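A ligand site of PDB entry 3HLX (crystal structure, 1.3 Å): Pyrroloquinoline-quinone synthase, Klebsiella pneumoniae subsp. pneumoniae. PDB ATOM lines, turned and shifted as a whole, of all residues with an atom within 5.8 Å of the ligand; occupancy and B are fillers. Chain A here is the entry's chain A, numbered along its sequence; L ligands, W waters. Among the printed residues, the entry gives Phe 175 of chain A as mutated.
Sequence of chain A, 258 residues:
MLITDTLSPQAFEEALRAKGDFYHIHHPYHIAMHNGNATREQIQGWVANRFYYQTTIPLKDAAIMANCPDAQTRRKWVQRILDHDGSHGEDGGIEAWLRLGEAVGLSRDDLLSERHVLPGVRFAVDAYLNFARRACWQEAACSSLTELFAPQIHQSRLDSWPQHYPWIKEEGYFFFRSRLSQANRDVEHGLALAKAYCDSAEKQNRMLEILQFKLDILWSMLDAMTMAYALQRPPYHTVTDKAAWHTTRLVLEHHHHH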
ATOM      1  N   TYR A  23     -13.575  41.633  -7.183  1.00  0.00           N
ATOM      2  CA  TYR A  23     -12.856  40.472  -6.675  1.00  0.00           C
ATOM      3  C   TYR A  23     -11.476  40.879  -6.093  1.00  0.00           C
ATOM      4  O   TYR A  23     -10.841  41.842  -6.555  1.00  0.00           O
ATOM      5  CB  TYR A  23     -12.672  39.373  -7.775  1.00  0.00           C
ATOM      6  CG  TYR A  23     -12.288  37.969  -7.347  1.00  0.00           C
ATOM      7  CD1 TYR A  23     -13.052  37.313  -6.391  1.00  0.00           C
ATOM      8  CD2 TYR A  23     -11.244  37.279  -7.967  1.00  0.00           C
ATOM      9  CE1 TYR A  23     -12.784  36.008  -6.027  1.00  0.00           C
ATOM     10  CE2 TYR A  23     -10.970  35.990  -7.616  1.00  0.00           C
ATOM     11  CZ  TYR A  23     -11.730  35.338  -6.677  1.00  0.00           C
ATOM     12  OH  TYR A  23     -11.483  34.082  -6.315  1.00  0.00           O
ATOM     13  N   HIS A  24     -10.980  40.055  -5.163  1.00  0.00           N
ATOM     14  CA  HIS A  24      -9.722  40.342  -4.462  1.00  0.00           C
ATOM     15  C   HIS A  24      -8.430  40.265  -5.336  1.00  0.00           C
ATOM     16  O   HIS A  24      -7.358  40.619  -4.848  1.00  0.00           O
ATOM     17  CB  HIS A  24      -9.566  39.503  -3.180  1.00  0.00           C
ATOM     18  CG  HIS A  24      -9.415  38.012  -3.316  1.00  0.00           C
ATOM     19  ND1 HIS A  24      -9.642  37.239  -4.452  1.00  0.00           N
ATOM     20  CD2 HIS A  24      -9.096  37.118  -2.336  1.00  0.00           C
ATOM     21  CE1 HIS A  24      -9.405  35.958  -4.163  1.00  0.00           C
ATOM     22  NE2 HIS A  24      -9.052  35.866  -2.900  1.00  0.00           N
ATOM     23  N   TRP A  46       0.650  34.999   4.158  1.00  0.00           N
ATOM     24  CA  TRP A  46      -0.540  34.712   3.323  1.00  0.00           C
ATOM     25  C   TRP A  46      -0.887  33.229   3.295  1.00  0.00           C
ATOM     26  O   TRP A  46      -2.055  32.837   3.451  1.00  0.00           O
ATOM     27  CB  TRP A  46      -0.350  35.333   1.926  1.00  0.00           C
ATOM     28  CG  TRP A  46      -1.465  35.104   0.932  1.00  0.00           C
ATOM     29  CD1 TRP A  46      -2.514  35.929   0.715  1.00  0.00           C
ATOM     30  CD2 TRP A  46      -1.584  34.025  -0.035  1.00  0.00           C
ATOM     31  NE1 TRP A  46      -3.350  35.400  -0.267  1.00  0.00           N
ATOM     32  CE2 TRP A  46      -2.773  34.239  -0.756  1.00  0.00           C
ATOM     33  CE3 TRP A  46      -0.825  32.884  -0.328  1.00  0.00           C
ATOM     34  CZ2 TRP A  46      -3.206  33.372  -1.771  1.00  0.00           C
ATOM     35  CZ3 TRP A  46      -1.272  32.023  -1.327  1.00  0.00           C
ATOM     36  CH2 TRP A  46      -2.439  32.291  -2.045  1.00  0.00           C
ATOM     37  N   ARG A  50      -4.317  32.007   4.893  1.00  0.00           N
ATOM     38  CA  ARG A  50      -5.287  31.403   3.974  1.00  0.00           C
ATOM     39  C   ARG A  50      -5.594  29.934   4.301  1.00  0.00           C
ATOM     40  O   ARG A  50      -6.712  29.439   3.981  1.00  0.00           O
ATOM     41  CB  ARG A  50      -4.824  31.494   2.498  1.00  0.00           C
ATOM     42  CG  ARG A  50      -5.402  32.740   1.810  1.00  0.00           C
ATOM     43  CD  ARG A  50      -6.940  32.617   1.525  1.00  0.00           C
ATOM     44  NE  ARG A  50      -7.161  31.488   0.645  1.00  0.00           N
ATOM     45  CZ  ARG A  50      -7.053  31.536  -0.664  1.00  0.00           C
ATOM     46  NH1 ARG A  50      -6.737  32.677  -1.282  1.00  0.00           N
ATOM     47  NH2 ARG A  50      -7.244  30.408  -1.386  1.00  0.00           N
ATOM     48  N   TYR A  53      -8.919  29.750   5.989  1.00  0.00           N
ATOM     49  CA  TYR A  53     -10.057  29.715   5.043  1.00  0.00           C
ATOM     50  C   TYR A  53     -10.208  28.298   4.447  1.00  0.00           C
ATOM     51  O   TYR A  53     -11.325  27.771   4.398  1.00  0.00           O
ATOM     52  CB  TYR A  53      -9.805  30.789   3.940  1.00  0.00           C
ATOM     53  CG  TYR A  53     -10.896  31.003   2.899  1.00  0.00           C
ATOM     54  CD1 TYR A  53     -12.049  31.672   3.226  1.00  0.00           C
ATOM     55  CD2 TYR A  53     -10.737  30.591   1.575  1.00  0.00           C
ATOM     56  CE1 TYR A  53     -13.041  31.905   2.302  1.00  0.00           C
ATOM     57  CE2 TYR A  53     -11.738  30.822   0.600  1.00  0.00           C
ATOM     58  CZ  TYR A  53     -12.893  31.484   0.997  1.00  0.00           C
ATOM     59  OH  TYR A  53     -13.953  31.749   0.092  1.00  0.00           O
ATOM     60  N   GLN A  54      -9.110  27.707   3.989  1.00  0.00           N
ATOM     61  CA  GLN A  54      -9.186  26.408   3.359  1.00  0.00           C
ATOM     62  C   GLN A  54      -9.768  25.345   4.273  1.00  0.00           C
ATOM     63  O   GLN A  54     -10.540  24.474   3.786  1.00  0.00           O
ATOM     64  CB  GLN A  54      -7.808  25.932   2.850  1.00  0.00           C
ATOM     65  CG  GLN A  54      -7.111  26.867   1.904  1.00  0.00           C
ATOM     66  CD  GLN A  54      -7.916  27.236   0.693  1.00  0.00           C
ATOM     67  OE1 GLN A  54      -8.449  26.365  -0.015  1.00  0.00           O
ATOM     68  NE2 GLN A  54      -7.983  28.512   0.430  1.00  0.00           N
ATOM     69  N   ILE A  57     -13.625  25.712   4.575  1.00  0.00           N
ATOM     70  CA  ILE A  57     -14.496  25.401   3.419  1.00  0.00           C
ATOM     71  C   ILE A  57     -15.334  24.133   3.724  1.00  0.00           C
ATOM     72  O   ILE A  57     -16.569  24.150   3.547  1.00  0.00           O
ATOM     73  CB  ILE A  57     -13.720  25.366   2.041  1.00  0.00           C
ATOM     74  CG1 ILE A  57     -13.145  26.769   1.753  1.00  0.00           C
ATOM     75  CG2 ILE A  57     -14.642  24.941   0.913  1.00  0.00           C
ATOM     76  CD1 ILE A  57     -14.171  27.939   1.748  1.00  0.00           C
ATOM     77  N   LYS A  60     -18.122  24.806   6.312  1.00  0.00           N
ATOM     78  CA  LYS A  60     -19.229  25.525   5.731  1.00  0.00           C
ATOM     79  C   LYS A  60     -20.047  24.727   4.746  1.00  0.00           C
ATOM     80  O   LYS A  60     -21.288  24.891   4.709  1.00  0.00           O
ATOM     81  CB  LYS A  60     -18.837  26.939   5.245  1.00  0.00           C
ATOM     82  CG  LYS A  60     -18.218  27.106   4.000  1.00  0.00           C
ATOM     83  CD  LYS A  60     -19.158  27.134   2.695  1.00  0.00           C
ATOM     84  CE  LYS A  60     -18.264  26.950   1.559  1.00  0.00           C
ATOM     85  NZ  LYS A  60     -19.053  26.842   0.314  1.00  0.00           N
ATOM     86  N   ASP A  61     -19.407  23.859   3.952  1.00  0.00           N
ATOM     87  CA  ASP A  61     -20.160  23.001   3.038  1.00  0.00           C
ATOM     88  C   ASP A  61     -20.998  21.939   3.832  1.00  0.00           C
ATOM     89  O   ASP A  61     -22.155  21.655   3.439  1.00  0.00           O
ATOM     90  CB  ASP A  61     -19.242  22.356   1.982  1.00  0.00           C
ATOM     91  CG  ASP A  61     -18.770  23.357   0.959  1.00  0.00           C
ATOM     92  OD1 ASP A  61     -19.631  24.150   0.539  1.00  0.00           O
ATOM     93  OD2 ASP A  61     -17.616  23.199   0.436  1.00  0.00           O
ATOM     94  N   ARG A  80     -17.680  18.595  -2.824  1.00  0.00           N
ATOM     95  CA  ARG A  80     -16.833  19.688  -2.340  1.00  0.00           C
ATOM     96  C   ARG A  80     -16.028  19.259  -1.098  1.00  0.00           C
ATOM     97  O   ARG A  80     -14.861  19.610  -0.943  1.00  0.00           O
ATOM     98  CB  ARG A  80     -17.655  20.987  -2.064  1.00  0.00           C
ATOM     99  CG  ARG A  80     -18.291  21.593  -3.302  1.00  0.00           C
ATOM    100  CD  ARG A  80     -19.508  22.412  -2.952  1.00  0.00           C
ATOM    101  NE  ARG A  80     -20.149  23.006  -4.132  1.00  0.00           N
ATOM    102  CZ  ARG A  80     -19.796  24.160  -4.679  1.00  0.00           C
ATOM    103  NH1 ARG A  80     -18.879  24.964  -4.098  1.00  0.00           N
ATOM    104  NH2 ARG A  80     -20.437  24.543  -5.808  1.00  0.00           N
ATOM    105  N   HIS A  84     -11.747  18.692  -0.735  1.00  0.00           N
ATOM    106  CA  HIS A  84     -10.845  19.229   0.246  1.00  0.00           C
ATOM    107  C   HIS A  84     -10.275  18.232   1.247  1.00  0.00           C
ATOM    108  O   HIS A  84      -9.074  18.336   1.637  1.00  0.00           O
ATOM    109  CB  HIS A  84     -11.507  20.447   0.954  1.00  0.00           C
ATOM    110  CG  HIS A  84     -11.446  21.697   0.103  1.00  0.00           C
ATOM    111  ND1 HIS A  84     -12.525  22.235  -0.552  1.00  0.00           N
ATOM    112  CD2 HIS A  84     -10.369  22.407  -0.319  1.00  0.00           C
ATOM    113  CE1 HIS A  84     -12.131  23.299  -1.262  1.00  0.00           C
ATOM    114  NE2 HIS A  84     -10.835  23.446  -1.114  1.00  0.00           N
ATOM    115  N   TRP A  97      -2.622  22.225   0.254  1.00  0.00           N
ATOM    116  CA  TRP A  97      -2.268  23.517   0.851  1.00  0.00           C
ATOM    117  C   TRP A  97      -1.096  23.363   1.844  1.00  0.00           C
ATOM    118  O   TRP A  97      -0.191  24.213   1.912  1.00  0.00           O
ATOM    119  CB  TRP A  97      -3.491  24.257   1.517  1.00  0.00           C
ATOM    120  CG  TRP A  97      -3.222  25.694   1.627  1.00  0.00           C
ATOM    121  CD1 TRP A  97      -2.582  26.340   2.668  1.00  0.00           C
ATOM    122  CD2 TRP A  97      -3.559  26.715   0.690  1.00  0.00           C
ATOM    123  NE1 TRP A  97      -2.491  27.699   2.410  1.00  0.00           N
ATOM    124  CE2 TRP A  97      -3.101  27.957   1.212  1.00  0.00           C
ATOM    125  CE3 TRP A  97      -4.245  26.717  -0.517  1.00  0.00           C
ATOM    126  CZ2 TRP A  97      -3.215  29.132   0.494  1.00  0.00           C
ATOM    127  CZ3 TRP A  97      -4.411  27.912  -1.208  1.00  0.00           C
ATOM    128  CH2 TRP A  97      -3.898  29.099  -0.689  1.00  0.00           C
ATOM    129  N   TYR A 128     -18.229  33.808   7.299  1.00  0.00           N
ATOM    130  CA  TYR A 128     -18.695  32.912   6.217  1.00  0.00           C
ATOM    131  C   TYR A 128     -19.364  31.640   6.736  1.00  0.00           C
ATOM    132  O   TYR A 128     -20.510  31.306   6.354  1.00  0.00           O
ATOM    133  CB  TYR A 128     -17.507  32.556   5.263  1.00  0.00           C
ATOM    134  CG  TYR A 128     -17.854  31.809   3.935  1.00  0.00           C
ATOM    135  CD1 TYR A 128     -19.113  31.948   3.347  1.00  0.00           C
ATOM    136  CD2 TYR A 128     -16.880  31.102   3.229  1.00  0.00           C
ATOM    137  CE1 TYR A 128     -19.383  31.319   2.112  1.00  0.00           C
ATOM    138  CE2 TYR A 128     -17.169  30.536   2.025  1.00  0.00           C
ATOM    139  CZ  TYR A 128     -18.396  30.670   1.462  1.00  0.00           C
ATOM    140  OH  TYR A 128     -18.751  30.106   0.248  1.00  0.00           O
ATOM    141  N   SER A 143     -23.601  31.719  -2.268  1.00  0.00           N
ATOM    142  CA  SER A 143     -22.480  32.554  -1.821  1.00  0.00           C
ATOM    143  C   SER A 143     -21.129  31.959  -2.142  1.00  0.00           C
ATOM    144  O   SER A 143     -20.105  32.649  -2.037  1.00  0.00           O
ATOM    145  CB  SER A 143     -22.587  32.859  -0.304  1.00  0.00           C
ATOM    146  OG  SER A 143     -22.321  31.737   0.556  1.00  0.00           O
ATOM    147  N   SER A 144     -21.121  30.725  -2.650  1.00  0.00           N
ATOM    148  CA  SER A 144     -19.897  30.084  -3.231  1.00  0.00           C
ATOM    149  C   SER A 144     -19.450  30.733  -4.539  1.00  0.00           C
ATOM    150  O   SER A 144     -18.349  30.492  -5.006  1.00  0.00           O
ATOM    151  CB  SER A 144     -20.074  28.568  -3.502  1.00  0.00           C
ATOM    152  OG  SER A 144     -21.065  28.399  -4.486  1.00  0.00           O
ATOM    153  N   LEU A 145     -20.309  31.548  -5.123  1.00  0.00           N
ATOM    154  CA  LEU A 145     -20.144  31.924  -6.558  1.00  0.00           C
ATOM    155  C   LEU A 145     -19.031  32.939  -6.826  1.00  0.00           C
ATOM    156  O   LEU A 145     -18.787  33.240  -8.009  1.00  0.00           O
ATOM    157  CB  LEU A 145     -21.450  32.346  -7.239  1.00  0.00           C
ATOM    158  CG  LEU A 145     -22.419  31.202  -7.646  1.00  0.00           C
ATOM    159  CD1 LEU A 145     -23.808  31.785  -8.010  1.00  0.00           C
ATOM    160  CD2 LEU A 145     -21.869  30.340  -8.798  1.00  0.00           C
ATOM    161  N   THR A 146     -18.306  33.417  -5.807  1.00  0.00           N
ATOM    162  CA  THR A 146     -16.999  34.029  -6.084  1.00  0.00           C
ATOM    163  C   THR A 146     -16.048  33.041  -6.803  1.00  0.00           C
ATOM    164  O   THR A 146     -15.088  33.458  -7.486  1.00  0.00           O
ATOM    165  CB  THR A 146     -16.315  34.652  -4.850  1.00  0.00           C
ATOM    166  OG1 THR A 146     -16.166  33.655  -3.814  1.00  0.00           O
ATOM    167  CG2 THR A 146     -17.134  35.888  -4.332  1.00  0.00           C
ATOM    168  N   GLU A 147     -16.303  31.704  -6.712  1.00  0.00           N
ATOM    169  CA  GLU A 147     -15.575  30.711  -7.526  1.00  0.00           C
ATOM    170  C   GLU A 147     -15.607  31.011  -9.027  1.00  0.00           C
ATOM    171  O   GLU A 147     -14.781  30.472  -9.809  1.00  0.00           O
ATOM    172  CB  GLU A 147     -16.113  29.316  -7.240  1.00  0.00           C
ATOM    173  CG  GLU A 147     -15.673  28.664  -5.912  1.00  0.00           C
ATOM    174  CD  GLU A 147     -16.214  27.274  -5.806  1.00  0.00           C
ATOM    175  OE1 GLU A 147     -17.447  27.105  -5.565  1.00  0.00           O
ATOM    176  OE2 GLU A 147     -15.344  26.353  -5.937  1.00  0.00           O
ATOM    177  N   ALA A 150     -12.288  32.581  -9.643  1.00  0.00           N
ATOM    178  CA  ALA A 150     -11.112  31.967  -9.039  1.00  0.00           C
ATOM    179  C   ALA A 150     -10.131  31.357 -10.081  1.00  0.00           C
ATOM    180  O   ALA A 150      -8.943  31.516  -9.914  1.00  0.00           O
ATOM    181  CB  ALA A 150     -11.541  30.942  -7.951  1.00  0.00           C
ATOM    182  N   ILE A 153      -7.557  33.909 -11.045  1.00  0.00           N
ATOM    183  CA  ILE A 153      -6.559  34.252 -10.022  1.00  0.00           C
ATOM    184  C   ILE A 153      -5.542  33.127  -9.818  1.00  0.00           C
ATOM    185  O   ILE A 153      -4.318  33.382  -9.685  1.00  0.00           O
ATOM    186  CB  ILE A 153      -7.177  34.797  -8.714  1.00  0.00           C
ATOM    187  CG1 ILE A 153      -6.192  35.713  -7.977  1.00  0.00           C
ATOM    188  CG2 ILE A 153      -7.765  33.657  -7.786  1.00  0.00           C
ATOM    189  CD1 ILE A 153      -6.759  36.440  -6.739  1.00  0.00           C
ATOM    190  N   HIS A 154      -6.018  31.888  -9.850  1.00  0.00           N
ATOM    191  CA  HIS A 154      -5.134  30.720  -9.727  1.00  0.00           C
ATOM    192  C   HIS A 154      -4.114  30.739 -10.894  1.00  0.00           C
ATOM    193  O   HIS A 154      -2.912  30.545 -10.690  1.00  0.00           O
ATOM    194  CB  HIS A 154      -5.908  29.399  -9.705  1.00  0.00           C
ATOM    195  CG  HIS A 154      -6.703  29.181  -8.461  1.00  0.00           C
ATOM    196  ND1 HIS A 154      -6.128  29.187  -7.219  1.00  0.00           N
ATOM    197  CD2 HIS A 154      -8.028  28.952  -8.288  1.00  0.00           C
ATOM    198  CE1 HIS A 154      -7.067  28.960  -6.317  1.00  0.00           C
ATOM    199  NE2 HIS A 154      -8.227  28.790  -6.944  1.00  0.00           N
ATOM    200  N   ARG A 157      -1.234  33.230 -10.623  1.00  0.00           N
ATOM    201  CA  ARG A 157      -0.121  32.801  -9.766  1.00  0.00           C
ATOM    202  C   ARG A 157       0.799  31.823 -10.467  1.00  0.00           C
ATOM    203  O   ARG A 157       2.025  31.923 -10.373  1.00  0.00           O
ATOM    204  CB  ARG A 157      -0.663  32.173  -8.488  1.00  0.00           C
ATOM    205  CG  ARG A 157      -1.558  33.135  -7.646  1.00  0.00           C
ATOM    206  CD  ARG A 157      -2.266  32.401  -6.432  1.00  0.00           C
ATOM    207  NE  ARG A 157      -3.228  33.296  -5.714  1.00  0.00           N
ATOM    208  CZ  ARG A 157      -4.480  33.008  -5.420  1.00  0.00           C
ATOM    209  NH1 ARG A 157      -4.976  31.796  -5.681  1.00  0.00           N
ATOM    210  NH2 ARG A 157      -5.221  33.926  -4.754  1.00  0.00           N
ATOM    211  N   PHE A 175      -1.922  22.746  -5.833  1.00  0.00           N
ATOM    212  CA  PHE A 175      -3.293  23.173  -5.408  1.00  0.00           C
ATOM    213  C   PHE A 175      -3.913  24.104  -6.463  1.00  0.00           C
ATOM    214  O   PHE A 175      -5.065  23.872  -6.924  1.00  0.00           O
ATOM    215  CB  PHE A 175      -3.350  23.810  -3.995  1.00  0.00           C
ATOM    216  CG  PHE A 175      -4.739  24.235  -3.611  1.00  0.00           C
ATOM    217  CD1 PHE A 175      -5.649  23.304  -3.124  1.00  0.00           C
ATOM    218  CD2 PHE A 175      -5.149  25.540  -3.744  1.00  0.00           C
ATOM    219  CE1 PHE A 175      -6.932  23.703  -2.793  1.00  0.00           C
ATOM    220  CE2 PHE A 175      -6.444  25.906  -3.415  1.00  0.00           C
ATOM    221  CZ  PHE A 175      -7.320  24.978  -2.944  1.00  0.00           C
ATOM    222  N   PHE A 176      -3.175  25.138  -6.876  1.00  0.00           N
ATOM    223  CA  PHE A 176      -3.725  26.121  -7.803  1.00  0.00           C
ATOM    224  C   PHE A 176      -4.108  25.441  -9.098  1.00  0.00           C
ATOM    225  O   PHE A 176      -5.151  25.745  -9.672  1.00  0.00           O
ATOM    226  CB  PHE A 176      -2.736  27.259  -8.102  1.00  0.00           C
ATOM    227  CG  PHE A 176      -2.231  28.010  -6.905  1.00  0.00           C
ATOM    228  CD1 PHE A 176      -3.024  28.368  -5.816  1.00  0.00           C
ATOM    229  CD2 PHE A 176      -0.923  28.427  -6.910  1.00  0.00           C
ATOM    230  CE1 PHE A 176      -2.469  29.059  -4.762  1.00  0.00           C
ATOM    231  CE2 PHE A 176      -0.371  29.154  -5.880  1.00  0.00           C
ATOM    232  CZ  PHE A 176      -1.160  29.465  -4.787  1.00  0.00           C
ATOM    233  N   ARG A 179      -7.433  23.460  -8.851  1.00  0.00           N
ATOM    234  CA  ARG A 179      -8.640  24.321  -8.792  1.00  0.00           C
ATOM    235  C   ARG A 179      -9.110  24.849 -10.132  1.00  0.00           C
ATOM    236  O   ARG A 179     -10.307  25.194 -10.289  1.00  0.00           O
ATOM    237  CB  ARG A 179      -8.464  25.443  -7.774  1.00  0.00           C
ATOM    238  CG  ARG A 179      -8.267  25.016  -6.324  1.00  0.00           C
ATOM    239  CD  ARG A 179      -9.367  24.100  -5.854  1.00  0.00           C
ATOM    240  NE  ARG A 179     -10.628  24.814  -5.780  1.00  0.00           N
ATOM    241  CZ  ARG A 179     -11.764  24.274  -5.401  1.00  0.00           C
ATOM    242  NH1 ARG A 179     -11.881  22.972  -5.109  1.00  0.00           N
ATOM    243  NH2 ARG A 179     -12.806  25.043  -5.320  1.00  0.00           N
ATOM    244  N   ASP A 186     -17.707  23.197  -9.931  1.00  0.00           N
ATOM    245  CA  ASP A 186     -18.502  23.759  -8.825  1.00  0.00           C
ATOM    246  C   ASP A 186     -19.532  24.799  -9.324  1.00  0.00           C
ATOM    247  O   ASP A 186     -20.728  24.763  -8.918  1.00  0.00           O
ATOM    248  CB  ASP A 186     -17.573  24.432  -7.753  1.00  0.00           C
ATOM    249  CG  ASP A 186     -16.848  23.426  -6.855  1.00  0.00           C
ATOM    250  OD1 ASP A 186     -17.089  22.223  -6.977  1.00  0.00           O
ATOM    251  OD2 ASP A 186     -15.974  23.851  -6.039  1.00  0.00           O
ATOM    252  N   LYS A 214     -19.740  38.233   0.548  1.00  0.00           N
ATOM    253  CA  LYS A 214     -18.662  37.263   0.277  1.00  0.00           C
ATOM    254  C   LYS A 214     -17.385  37.943  -0.230  1.00  0.00           C
ATOM    255  O   LYS A 214     -16.276  37.681   0.259  1.00  0.00           O
ATOM    256  CB  LYS A 214     -19.121  36.216  -0.705  1.00  0.00           C
ATOM    257  CG  LYS A 214     -18.075  35.166  -1.082  1.00  0.00           C
ATOM    258  CD  LYS A 214     -17.688  34.261   0.044  1.00  0.00           C
ATOM    259  CE  LYS A 214     -16.736  33.126  -0.425  1.00  0.00           C
ATOM    260  NZ  LYS A 214     -17.131  32.274  -1.639  1.00  0.00           N
ATOM    261  N   LEU A 218     -13.362  38.315   1.546  1.00  0.00           N
ATOM    262  CA  LEU A 218     -12.084  38.147   0.918  1.00  0.00           C
ATOM    263  C   LEU A 218     -11.193  39.385   1.023  1.00  0.00           C
ATOM    264  O   LEU A 218      -9.999  39.304   1.354  1.00  0.00           O
ATOM    265  CB  LEU A 218     -12.270  37.763  -0.560  1.00  0.00           C
ATOM    266  CG  LEU A 218     -12.978  36.428  -0.863  1.00  0.00           C
ATOM    267  CD1 LEU A 218     -13.126  36.204  -2.394  1.00  0.00           C
ATOM    268  CD2 LEU A 218     -12.281  35.200  -0.234  1.00  0.00           C
HETATM  269  N1  LIG L   1     -14.264  29.541  -2.525  1.00  0.00           N
HETATM  270  C1  LIG L   1     -14.937  28.397  -2.177  1.00  0.00           C
HETATM  271  C2  LIG L   1     -16.372  28.429  -1.748  1.00  0.00           C
HETATM  272  O1  LIG L   1     -16.823  29.584  -1.478  1.00  0.00           O
HETATM  273  O2  LIG L   1     -16.932  27.361  -1.444  1.00  0.00           O
HETATM  274  C3  LIG L   1     -14.055  27.314  -2.159  1.00  0.00           C
HETATM  275  C4  LIG L   1     -12.744  27.800  -2.536  1.00  0.00           C
HETATM  276  C5  LIG L   1     -12.939  29.240  -2.811  1.00  0.00           C
HETATM  277  C6  LIG L   1     -11.435  27.177  -2.631  1.00  0.00           C
HETATM  278  O3  LIG L   1     -11.234  25.912  -2.474  1.00  0.00           O
HETATM  279  C7  LIG L   1     -10.307  28.027  -2.998  1.00  0.00           C
HETATM  280  O4  LIG L   1      -9.091  27.562  -3.110  1.00  0.00           O
HETATM  281  C8  LIG L   1     -10.561  29.475  -3.285  1.00  0.00           C
HETATM  282  N2  LIG L   1      -9.477  30.186  -3.656  1.00  0.00           N
HETATM  283  C9  LIG L   1      -9.544  31.481  -3.939  1.00  0.00           C
HETATM  284  C10 LIG L   1      -8.234  32.177  -4.255  1.00  0.00           C
HETATM  285  O5  LIG L   1      -7.202  31.439  -4.171  1.00  0.00           O
HETATM  286  O6  LIG L   1      -8.239  33.418  -4.461  1.00  0.00           O
HETATM  287  C11 LIG L   1     -10.743  32.191  -3.809  1.00  0.00           C
HETATM  288  C12 LIG L   1     -11.949  31.556  -3.464  1.00  0.00           C
HETATM  289  C13 LIG L   1     -13.198  32.348  -3.482  1.00  0.00           C
HETATM  290  O7  LIG L   1     -13.361  33.103  -4.522  1.00  0.00           O
HETATM  291  O8  LIG L   1     -14.096  32.160  -2.630  1.00  0.00           O
HETATM  292  C14 LIG L   1     -11.885  30.104  -3.174  1.00  0.00           C
HETATM  293  O   HOH W   1     -16.986  24.673  -1.861  1.00  0.00           O
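The side-chain hydroxyl (OH) of Tyr 23 sits at hydrogen-bond distance from an oxygen (O7) of the ligand (2.8 Å).
O8 of the ligand lies within hydrogen-bond range of OG1 of Thr 146, 2.8 Å away.
O5 of the ligand lies within salt-bridge range of NH1 of Arg 157, 2.7 Å away.
The side-chain amino group (NZ) of Lys 214 is in salt-bridge range of an oxygen (O1) of the ligand (2.7 Å).
The guanidinium group (NH2) of Arg 179 is in hydrogen-bond range of an oxygen (O3) of the ligand, at 3.4 Å.
NH2 of Arg 50 lies within salt-bridge range of O5 of the ligand.
An oxygen (O1) of the ligand is in hydrogen-bond range of the side-chain hydroxyl (OH) of Tyr 128.
An oxygen (O2) of the ligand lies within salt-bridge range of the side-chain amino group (NZ) of Lys 60, at 2.8 Å.
An oxygen (O6) of the ligand lies close to a ring nitrogen (NE2) of His 24.
OH of Tyr 53 lies within hydrogen-bond range of O8 of the ligand.
O3 of the ligand sits at hydrogen-bond distance from NE2 of His 84, 2.8 Å away.
OE1 of Gln 54 lies close to O4 of the ligand (3.4 Å).
NH1 of Arg 80 lies within salt-bridge range of OE1 of Glu 147 (3.0 Å).
The side-chain amino group (NZ) of Lys 214 lies within hydrogen-bond range of the side-chain hydroxyl (OG1) of Thr 146 (2.8 Å).
The side-chain amino group (NZ) of Lys 60 lies within salt-bridge range of the side-chain carboxylate (OD1) of Asp 61, 2.8 Å away.
The side-chain hydroxyl of Tyr 128 is in hydrogen-bond range of the side-chain amino group of Lys 214 (3.3 Å).
The side-chain carboxylate of Glu 147 sits close to the side-chain carboxylate of Asp 186.
The side-chain amide nitrogen of Gln 54 lies close to the guanidinium group of Arg 50 (2.7 Å).
The guanidinium group (NH1) of Arg 157 lies within hydrogen-bond range of a ring nitrogen (ND1) of His 154 (3.2 Å).
The side-chain carboxylate (OD2) of Asp 186 lies within salt-bridge range of the guanidinium group (NH2) of Arg 179 (3.5 Å).
Residues that only touch the ligand: Ile 57 (3.9 Å), Ser 144 (3.6 Å), Glu 147 (3.8 Å), Ile 153 (3.4 Å), His 154 (3.3 Å), Phe 175 (3.1 Å) and Leu 218 (3.8 Å).
Of the 28 residues printed, 19 come within 4 Å of the ligand.
Water W1 lies within hydrogen-bond range of O2 of the ligand (2.7 Å), OD2 of Asp 61 (2.8 Å) and NH1 of Arg 80 (2.9 Å).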
